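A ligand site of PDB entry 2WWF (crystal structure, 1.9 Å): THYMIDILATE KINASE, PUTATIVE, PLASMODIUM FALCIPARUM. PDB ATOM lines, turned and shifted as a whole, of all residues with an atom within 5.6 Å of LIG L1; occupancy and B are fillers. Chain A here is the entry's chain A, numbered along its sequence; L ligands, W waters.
Merely in contact with LIG L1: Ser 148 (3.9 Å), Ile 186 (3.4 Å) and Ile 189 (3.8 Å).
Hydrophobic or aromatic side chains within 4 Å of LIG L1: Ile 186 and Ile 189.
11 residues have an atom within 4 Å of LIG L1: Arg 20, Ser 21, Gly 22, Lys 23, Ser 24, Thr 25, Arg 147, Ser 148, Arg 184, Ile 186 and Ile 189.
The nearest printed residue that does not touch LIG L1 is Lys 185 (4.1 Å).
Water W7 lies within hydrogen-bond range of an oxygen (O5) of LIG L1 (2.6 Å) and the side-chain hydroxyl (OG) of Ser 24 (2.7 Å).
Water W10 lies within hydrogen-bond range of O10 of LIG L1 and OG1 of Thr 25.
Water W5 lies within hydrogen-bond range of N2 of LIG L1 (2.8 Å) and NE2 of Gln 26 (3.0 Å).
Water W2 bridges N4 of LIG L1 and N of Ile 186.
Water W6 lies within hydrogen-bond range of an oxygen (O3) of LG2 L2 (2.7 Å) and an oxygen (O3) of LIG L1 (3.3 Å).
Water W4 lies within hydrogen-bond range of O of Ser 21, O of Ala 182, NH1 of Arg 147 and N3 of LIG L1.
An oxygen (O4) of LIG L1 is in hydrogen-bond range of the backbone NH (N) of Thr 25 (2.8 Å).
OG1 of Thr 25 is in hydrogen-bond range of O4 of LIG L1 (2.6 Å).
An oxygen (O2) of LIG L1 sits at hydrogen-bond distance from the backbone NH (N) of Lys 23 (2.8 Å).
The side-chain amino group (NZ) of Lys 23 lies within salt-bridge range of an oxygen (O2) of LIG L1, at 2.7 Å.
An oxygen (O1) of LIG L1 sits at hydrogen-bond distance from the backbone NH (N) of Ser 24, 2.8 Å away.
OG of Ser 24 is in hydrogen-bond range of O1 of LIG L1 (3.1 Å).
A nitrogen (N3) of LIG L1 is in hydrogen-bond range of the backbone carbonyl oxygen of Arg 184 (3.0 Å).
The backbone NH (N) of Gly 22 lies within hydrogen-bond range of an oxygen (O2) of LIG L1, at 3.0 Å.
The backbone NH (N) of Ser 21 sits at hydrogen-bond distance from an oxygen (O2) of LIG L1, at 3.2 Å.
N of Arg 20 sits at hydrogen-bond distance from O3 of LIG L1 (3.2 Å).
A nitrogen (N4) of LIG L1 lies close to the guanidinium group (NH2) of Arg 147 (3.4 Å).
The side-chain carboxylate (OD1) of Asp 19 lies within hydrogen-bond range of an oxygen (O6) of LG2 L2, 2.8 Å away.
NE of Arg 101 lies within salt-bridge range of O1 of LG2 L2 (2.7 Å).
NZ of Lys 23 sits at hydrogen-bond distance from O of Leu 18 (3.3 Å).
The guanidinium group (NH1) of Arg 147 sits at hydrogen-bond distance from the backbone carbonyl oxygen (O) of Ser 21 (3.4 Å).
OG of Ser 21 sits at hydrogen-bond distance from O of Leu 18, 2.7 Å away.
The guanidinium group (NH1) of Arg 147 sits at hydrogen-bond distance from the backbone carbonyl oxygen (O) of Arg 20.
NH2 of Arg 147 is in hydrogen-bond range of OH of Tyr 143, at 3.3 Å.
The backbone carbonyl oxygen (O) of Ile 186 is in hydrogen-bond range of the side-chain amide nitrogen (NE2) of Gln 26 (3.2 Å).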
ATOM      1  N   LEU A  18      12.244  18.883 -33.676  1.00  0.00           N
ATOM      2  CA  LEU A  18      13.384  19.425 -32.967  1.00  0.00           C
ATOM      3  C   LEU A  18      13.412  19.013 -31.494  1.00  0.00           C
ATOM      4  O   LEU A  18      12.458  18.414 -31.000  1.00  0.00           O
ATOM      5  CB  LEU A  18      13.411  20.972 -33.105  1.00  0.00           C
ATOM      6  CG  LEU A  18      13.769  21.450 -34.537  1.00  0.00           C
ATOM      7  CD1 LEU A  18      13.814  23.030 -34.508  1.00  0.00           C
ATOM      8  CD2 LEU A  18      15.170  20.931 -34.981  1.00  0.00           C
ATOM      9  N   ASP A  19      14.504  19.324 -30.764  1.00  0.00           N
ATOM     10  CA  ASP A  19      14.586  19.016 -29.349  1.00  0.00           C
ATOM     11  C   ASP A  19      13.480  19.737 -28.521  1.00  0.00           C
ATOM     12  O   ASP A  19      13.294  20.918 -28.698  1.00  0.00           O
ATOM     13  CB  ASP A  19      15.980  19.378 -28.892  1.00  0.00           C
ATOM     14  CG  ASP A  19      17.006  18.399 -29.495  1.00  0.00           C
ATOM     15  OD1 ASP A  19      17.199  17.313 -28.886  1.00  0.00           O
ATOM     16  OD2 ASP A  19      17.428  18.650 -30.652  1.00  0.00           O
ATOM     17  N   ARG A  20      12.763  18.990 -27.675  1.00  0.00           N
ATOM     18  CA  ARG A  20      11.749  19.545 -26.787  1.00  0.00           C
ATOM     19  C   ARG A  20      10.524  20.038 -27.573  1.00  0.00           C
ATOM     20  O   ARG A  20       9.779  20.902 -27.060  1.00  0.00           O
ATOM     21  CB  ARG A  20      12.334  20.723 -25.963  1.00  0.00           C
ATOM     22  CG  ARG A  20      13.065  20.363 -24.673  1.00  0.00           C
ATOM     23  CD  ARG A  20      14.324  19.580 -24.715  1.00  0.00           C
ATOM     24  NE  ARG A  20      14.209  18.762 -23.525  1.00  0.00           N
ATOM     25  CZ  ARG A  20      15.150  18.418 -22.660  1.00  0.00           C
ATOM     26  NH1 ARG A  20      16.438  18.757 -22.741  1.00  0.00           N
ATOM     27  NH2 ARG A  20      14.764  17.691 -21.642  1.00  0.00           N
ATOM     28  N   SER A  21      10.293  19.518 -28.778  1.00  0.00           N
ATOM     29  CA  SER A  21       9.206  19.995 -29.603  1.00  0.00           C
ATOM     30  C   SER A  21       7.865  19.347 -29.123  1.00  0.00           C
ATOM     31  O   SER A  21       6.800  19.706 -29.623  1.00  0.00           O
ATOM     32  CB  SER A  21       9.454  19.719 -31.113  1.00  0.00           C
ATOM     33  OG  SER A  21       9.758  18.302 -31.328  1.00  0.00           O
ATOM     34  N   GLY A  22       7.895  18.397 -28.158  1.00  0.00           N
ATOM     35  CA  GLY A  22       6.680  17.716 -27.685  1.00  0.00           C
ATOM     36  C   GLY A  22       6.449  16.295 -28.143  1.00  0.00           C
ATOM     37  O   GLY A  22       5.313  15.754 -28.054  1.00  0.00           O
ATOM     38  N   LYS A  23       7.499  15.602 -28.634  1.00  0.00           N
ATOM     39  CA  LYS A  23       7.324  14.227 -29.129  1.00  0.00           C
ATOM     40  C   LYS A  23       6.897  13.230 -28.031  1.00  0.00           C
ATOM     41  O   LYS A  23       5.949  12.468 -28.241  1.00  0.00           O
ATOM     42  CB  LYS A  23       8.653  13.730 -29.862  1.00  0.00           C
ATOM     43  CG  LYS A  23       8.950  14.504 -31.156  1.00  0.00           C
ATOM     44  CD  LYS A  23      10.315  14.025 -31.808  1.00  0.00           C
ATOM     45  CE  LYS A  23      11.504  14.878 -31.363  1.00  0.00           C
ATOM     46  NZ  LYS A  23      11.699  15.338 -29.992  1.00  0.00           N
ATOM     47  N   SER A  24       7.561  13.218 -26.878  1.00  0.00           N
ATOM     48  CA  SER A  24       7.162  12.268 -25.780  1.00  0.00           C
ATOM     49  C   SER A  24       5.700  12.577 -25.359  1.00  0.00           C
ATOM     50  O   SER A  24       4.900  11.634 -25.156  1.00  0.00           O
ATOM     51  CB  SER A  24       8.014  12.432 -24.517  1.00  0.00           C
ATOM     52  OG  SER A  24       9.368  12.024 -24.776  1.00  0.00           O
ATOM     53  N   THR A  25       5.409  13.865 -25.224  1.00  0.00           N
ATOM     54  CA  THR A  25       4.008  14.345 -24.890  1.00  0.00           C
ATOM     55  C   THR A  25       2.910  13.785 -25.828  1.00  0.00           C
ATOM     56  O   THR A  25       1.921  13.149 -25.378  1.00  0.00           O
ATOM     57  CB  THR A  25       3.972  15.914 -24.854  1.00  0.00           C
ATOM     58  OG1 THR A  25       4.877  16.348 -23.837  1.00  0.00           O
ATOM     59  CG2 THR A  25       2.493  16.453 -24.483  1.00  0.00           C
ATOM     60  N   GLN A  26       3.114  14.004 -27.129  1.00  0.00           N
ATOM     61  CA  GLN A  26       2.227  13.566 -28.183  1.00  0.00           C
ATOM     62  C   GLN A  26       2.183  12.046 -28.403  1.00  0.00           C
ATOM     63  O   GLN A  26       1.099  11.479 -28.593  1.00  0.00           O
ATOM     64  CB  GLN A  26       2.563  14.314 -29.498  1.00  0.00           C
ATOM     65  CG  GLN A  26       2.305  15.843 -29.397  1.00  0.00           C
ATOM     66  CD  GLN A  26       0.830  16.175 -29.021  1.00  0.00           C
ATOM     67  OE1 GLN A  26      -0.087  15.447 -29.415  1.00  0.00           O
ATOM     68  NE2 GLN A  26       0.623  17.291 -28.269  1.00  0.00           N
ATOM     69  N   ARG A 101      11.072   9.340 -32.554  1.00  0.00           N
ATOM     70  CA  ARG A 101      12.325   9.452 -33.401  1.00  0.00           C
ATOM     71  C   ARG A 101      12.624   8.168 -34.121  1.00  0.00           C
ATOM     72  O   ARG A 101      12.361   7.076 -33.625  1.00  0.00           O
ATOM     73  CB  ARG A 101      13.604   9.928 -32.610  1.00  0.00           C
ATOM     74  CG  ARG A 101      13.487  11.344 -32.053  1.00  0.00           C
ATOM     75  CD  ARG A 101      14.892  11.798 -31.513  1.00  0.00           C
ATOM     76  NE  ARG A 101      14.886  13.130 -30.878  1.00  0.00           N
ATOM     77  CZ  ARG A 101      14.855  14.252 -31.546  1.00  0.00           C
ATOM     78  NH1 ARG A 101      14.747  14.233 -32.919  1.00  0.00           N
ATOM     79  NH2 ARG A 101      14.824  15.364 -30.837  1.00  0.00           N
ATOM     80  N   TYR A 143      12.000  28.323 -30.873  1.00  0.00           N
ATOM     81  CA  TYR A 143      10.733  28.272 -30.146  1.00  0.00           C
ATOM     82  C   TYR A 143      10.790  27.560 -28.816  1.00  0.00           C
ATOM     83  O   TYR A 143      10.241  28.083 -27.848  1.00  0.00           O
ATOM     84  CB  TYR A 143       9.652  27.705 -31.057  1.00  0.00           C
ATOM     85  CG  TYR A 143       8.358  27.354 -30.318  1.00  0.00           C
ATOM     86  CD1 TYR A 143       7.388  28.323 -30.090  1.00  0.00           C
ATOM     87  CD2 TYR A 143       8.121  26.044 -29.860  1.00  0.00           C
ATOM     88  CE1 TYR A 143       6.155  27.967 -29.391  1.00  0.00           C
ATOM     89  CE2 TYR A 143       6.927  25.693 -29.172  1.00  0.00           C
ATOM     90  CZ  TYR A 143       5.947  26.687 -28.959  1.00  0.00           C
ATOM     91  OH  TYR A 143       4.790  26.386 -28.273  1.00  0.00           O
ATOM     92  N   ARG A 147      11.567  25.532 -22.718  1.00  0.00           N
ATOM     93  CA  ARG A 147      10.871  24.377 -22.124  1.00  0.00           C
ATOM     94  C   ARG A 147      11.818  23.632 -21.248  1.00  0.00           C
ATOM     95  O   ARG A 147      13.031  23.695 -21.480  1.00  0.00           O
ATOM     96  CB  ARG A 147      10.250  23.473 -23.209  1.00  0.00           C
ATOM     97  CG  ARG A 147       9.664  24.282 -24.357  1.00  0.00           C
ATOM     98  CD  ARG A 147       8.159  24.342 -24.570  1.00  0.00           C
ATOM     99  NE  ARG A 147       7.917  23.348 -25.562  1.00  0.00           N
ATOM    100  CZ  ARG A 147       6.904  23.117 -26.391  1.00  0.00           C
ATOM    101  NH1 ARG A 147       7.050  22.026 -27.141  1.00  0.00           N
ATOM    102  NH2 ARG A 147       5.786  23.830 -26.524  1.00  0.00           N
ATOM    103  N   SER A 148      11.269  22.898 -20.281  1.00  0.00           N
ATOM    104  CA  SER A 148      11.982  22.465 -19.081  1.00  0.00           C
ATOM    105  C   SER A 148      13.536  22.288 -19.152  1.00  0.00           C
ATOM    106  O   SER A 148      14.290  23.194 -18.834  1.00  0.00           O
ATOM    107  CB  SER A 148      11.281  21.293 -18.393  1.00  0.00           C
ATOM    108  N   ALA A 182       3.330  22.613 -34.239  1.00  0.00           N
ATOM    109  CA  ALA A 182       3.432  22.175 -32.841  1.00  0.00           C
ATOM    110  C   ALA A 182       3.656  23.360 -31.917  1.00  0.00           C
ATOM    111  O   ALA A 182       4.036  23.176 -30.781  1.00  0.00           O
ATOM    112  CB  ALA A 182       4.560  21.078 -32.699  1.00  0.00           C
ATOM    113  N   ARG A 184       1.251  25.120 -30.841  1.00  0.00           N
ATOM    114  CA  ARG A 184      -0.106  25.250 -30.296  1.00  0.00           C
ATOM    115  C   ARG A 184      -0.274  24.514 -28.967  1.00  0.00           C
ATOM    116  O   ARG A 184       0.650  23.838 -28.466  1.00  0.00           O
ATOM    117  CB  ARG A 184      -1.106  24.775 -31.337  1.00  0.00           C
ATOM    118  CG  ARG A 184      -1.102  25.666 -32.640  1.00  0.00           C
ATOM    119  CD  ARG A 184      -1.983  25.090 -33.673  1.00  0.00           C
ATOM    120  NE  ARG A 184      -1.501  23.790 -34.129  1.00  0.00           N
ATOM    121  CZ  ARG A 184      -2.292  22.786 -34.484  1.00  0.00           C
ATOM    122  NH1 ARG A 184      -3.639  22.932 -34.462  1.00  0.00           N
ATOM    123  NH2 ARG A 184      -1.745  21.652 -34.911  1.00  0.00           N
ATOM    124  N   LYS A 185      -1.464  24.597 -28.388  1.00  0.00           N
ATOM    125  CA  LYS A 185      -1.808  23.829 -27.206  1.00  0.00           C
ATOM    126  C   LYS A 185      -1.715  22.320 -27.495  1.00  0.00           C
ATOM    127  O   LYS A 185      -2.046  21.859 -28.577  1.00  0.00           O
ATOM    128  CB  LYS A 185      -3.304  24.102 -26.815  1.00  0.00           C
ATOM    129  CG  LYS A 185      -3.604  25.423 -26.198  1.00  0.00           C
ATOM    130  CD  LYS A 185      -5.105  25.476 -25.833  1.00  0.00           C
ATOM    131  CE  LYS A 185      -5.849  26.362 -26.833  1.00  0.00           C
ATOM    132  NZ  LYS A 185      -6.767  25.666 -27.801  1.00  0.00           N
ATOM    133  N   ILE A 186      -1.365  21.581 -26.457  1.00  0.00           N
ATOM    134  CA  ILE A 186      -1.151  20.138 -26.513  1.00  0.00           C
ATOM    135  C   ILE A 186      -2.385  19.458 -27.136  1.00  0.00           C
ATOM    136  O   ILE A 186      -2.307  18.635 -28.085  1.00  0.00           O
ATOM    137  CB  ILE A 186      -0.874  19.636 -25.058  1.00  0.00           C
ATOM    138  CG1 ILE A 186       0.568  20.005 -24.626  1.00  0.00           C
ATOM    139  CG2 ILE A 186      -1.096  18.135 -24.930  1.00  0.00           C
ATOM    140  CD1 ILE A 186       0.900  19.764 -23.145  1.00  0.00           C
ATOM    141  N   ILE A 189      -2.846  20.039 -31.001  1.00  0.00           N
ATOM    142  CA  ILE A 189      -1.907  19.196 -31.704  1.00  0.00           C
ATOM    143  C   ILE A 189      -2.428  17.757 -31.694  1.00  0.00           C
ATOM    144  O   ILE A 189      -2.468  17.106 -32.716  1.00  0.00           O
ATOM    145  CB  ILE A 189      -0.503  19.298 -31.071  1.00  0.00           C
ATOM    146  CG1 ILE A 189       0.050  20.743 -31.248  1.00  0.00           C
ATOM    147  CG2 ILE A 189       0.553  18.282 -31.701  1.00  0.00           C
ATOM    148  CD1 ILE A 189       1.203  20.978 -30.295  1.00  0.00           C
HETATM  149  P1  LIG L   1      10.416  15.929 -26.712  1.00  0.00           P
HETATM  150  O1  LIG L   1       9.953  14.585 -26.381  1.00  0.00           O
HETATM  151  O2  LIG L   1      10.138  16.418 -28.123  1.00  0.00           O
HETATM  152  O3  LIG L   1      11.796  16.224 -26.289  1.00  0.00           O
HETATM  153  P2  LIG L   1       8.511  16.597 -24.588  1.00  0.00           P
HETATM  154  O4  LIG L   1       7.226  15.993 -24.973  1.00  0.00           O
HETATM  155  O5  LIG L   1       9.291  15.964 -23.467  1.00  0.00           O
HETATM  156  O6  LIG L   1       9.505  16.983 -25.812  1.00  0.00           O
HETATM  157  O7  LIG L   1       8.200  18.120 -24.126  1.00  0.00           O
HETATM  158  C1  LIG L   1       9.217  19.051 -23.661  1.00  0.00           C
HETATM  159  C2  LIG L   1       8.592  19.977 -22.571  1.00  0.00           C
HETATM  160  O8  LIG L   1       7.556  20.765 -23.167  1.00  0.00           O
HETATM  161  C3  LIG L   1       7.932  19.178 -21.467  1.00  0.00           C
HETATM  162  O9  LIG L   1       8.136  19.876 -20.257  1.00  0.00           O
HETATM  163  C4  LIG L   1       6.470  19.171 -21.870  1.00  0.00           C
HETATM  164  O10 LIG L   1       5.578  19.072 -20.776  1.00  0.00           O
HETATM  165  C5  LIG L   1       6.296  20.509 -22.512  1.00  0.00           C
HETATM  166  N1  LIG L   1       5.390  20.551 -23.656  1.00  0.00           N
HETATM  167  C6  LIG L   1       5.239  19.632 -24.663  1.00  0.00           C
HETATM  168  N2  LIG L   1       4.322  20.069 -25.597  1.00  0.00           N
HETATM  169  C7  LIG L   1       3.887  21.287 -25.158  1.00  0.00           C
HETATM  170  C8  LIG L   1       2.931  22.281 -25.660  1.00  0.00           C
HETATM  171  N3  LIG L   1       2.350  22.026 -26.857  1.00  0.00           N
HETATM  172  N4  LIG L   1       2.775  23.427 -24.930  1.00  0.00           N
HETATM  173  C9  LIG L   1       3.437  23.647 -23.779  1.00  0.00           C
HETATM  174  N5  LIG L   1       4.298  22.757 -23.251  1.00  0.00           N
HETATM  175  C10 LIG L   1       4.573  21.597 -23.904  1.00  0.00           C
HETATM  176  P1  LG2 L   2      15.825  12.968 -27.272  1.00  0.00           P
HETATM  177  O1  LG2 L   2      15.100  12.428 -28.321  1.00  0.00           O
HETATM  178  O2  LG2 L   2      15.918  14.372 -27.615  1.00  0.00           O
HETATM  179  O3  LG2 L   2      15.652  13.064 -25.906  1.00  0.00           O
HETATM  180  O4  LG2 L   2      17.513  12.935 -27.518  1.00  0.00           O
HETATM  181  C1  LG2 L   2      18.074  12.391 -28.627  1.00  0.00           C
HETATM  182  C2  LG2 L   2      19.132  13.327 -29.185  1.00  0.00           C
HETATM  183  O5  LG2 L   2      19.745  12.492 -30.212  1.00  0.00           O
HETATM  184  C3  LG2 L   2      18.362  14.399 -29.974  1.00  0.00           C
HETATM  185  O6  LG2 L   2      19.153  15.641 -29.950  1.00  0.00           O
HETATM  186  C4  LG2 L   2      18.263  13.876 -31.431  1.00  0.00           C
HETATM  187  C5  LG2 L   2      19.613  13.121 -31.513  1.00  0.00           C
HETATM  188  N1  LG2 L   2      19.578  11.969 -32.455  1.00  0.00           N
HETATM  189  C6  LG2 L   2      20.560  11.860 -33.443  1.00  0.00           C
HETATM  190  O7  LG2 L   2      21.465  12.700 -33.579  1.00  0.00           O
HETATM  191  N2  LG2 L   2      20.544  10.782 -34.373  1.00  0.00           N
HETATM  192  C7  LG2 L   2      19.528   9.819 -34.265  1.00  0.00           C
HETATM  193  O8  LG2 L   2      19.587   8.911 -35.075  1.00  0.00           O
HETATM  194  C8  LG2 L   2      18.548   9.921 -33.284  1.00  0.00           C
HETATM  195  C9  LG2 L   2      17.396   8.811 -33.122  1.00  0.00           C
HETATM  196  C10 LG2 L   2      18.564  10.989 -32.374  1.00  0.00           C
HETATM  197  O   HOH W   1       8.116  15.169 -21.196  1.00  0.00           O
HETATM  198  O   HOH W   2      -0.149  23.325 -24.222  1.00  0.00           O
HETATM  199  O   HOH W   3      12.357  16.449 -23.498  1.00  0.00           O
HETATM  200  O   HOH W   4       4.713  21.210 -29.017  1.00  0.00           O
HETATM  201  O   HOH W   5       3.068  18.955 -27.836  1.00  0.00           O
HETATM  202  O   HOH W   6      13.036  13.409 -25.197  1.00  0.00           O
HETATM  203  O   HOH W   7      10.753  13.877 -23.343  1.00  0.00           O
HETATM  204  O   HOH W   8       6.097  23.972 -21.416  1.00  0.00           O
HETATM  205  O   HOH W   9       8.454  22.822 -20.404  1.00  0.00           O
HETATM  206  O   HOH W  10       3.951  17.048 -21.203  1.00  0.00           O
HETATM  207  O   HOH W  11      13.798  15.946 -27.926  1.00  0.00           O
HETATM  208  O   HOH W  12       7.358  18.851 -18.051  1.00  0.00           O
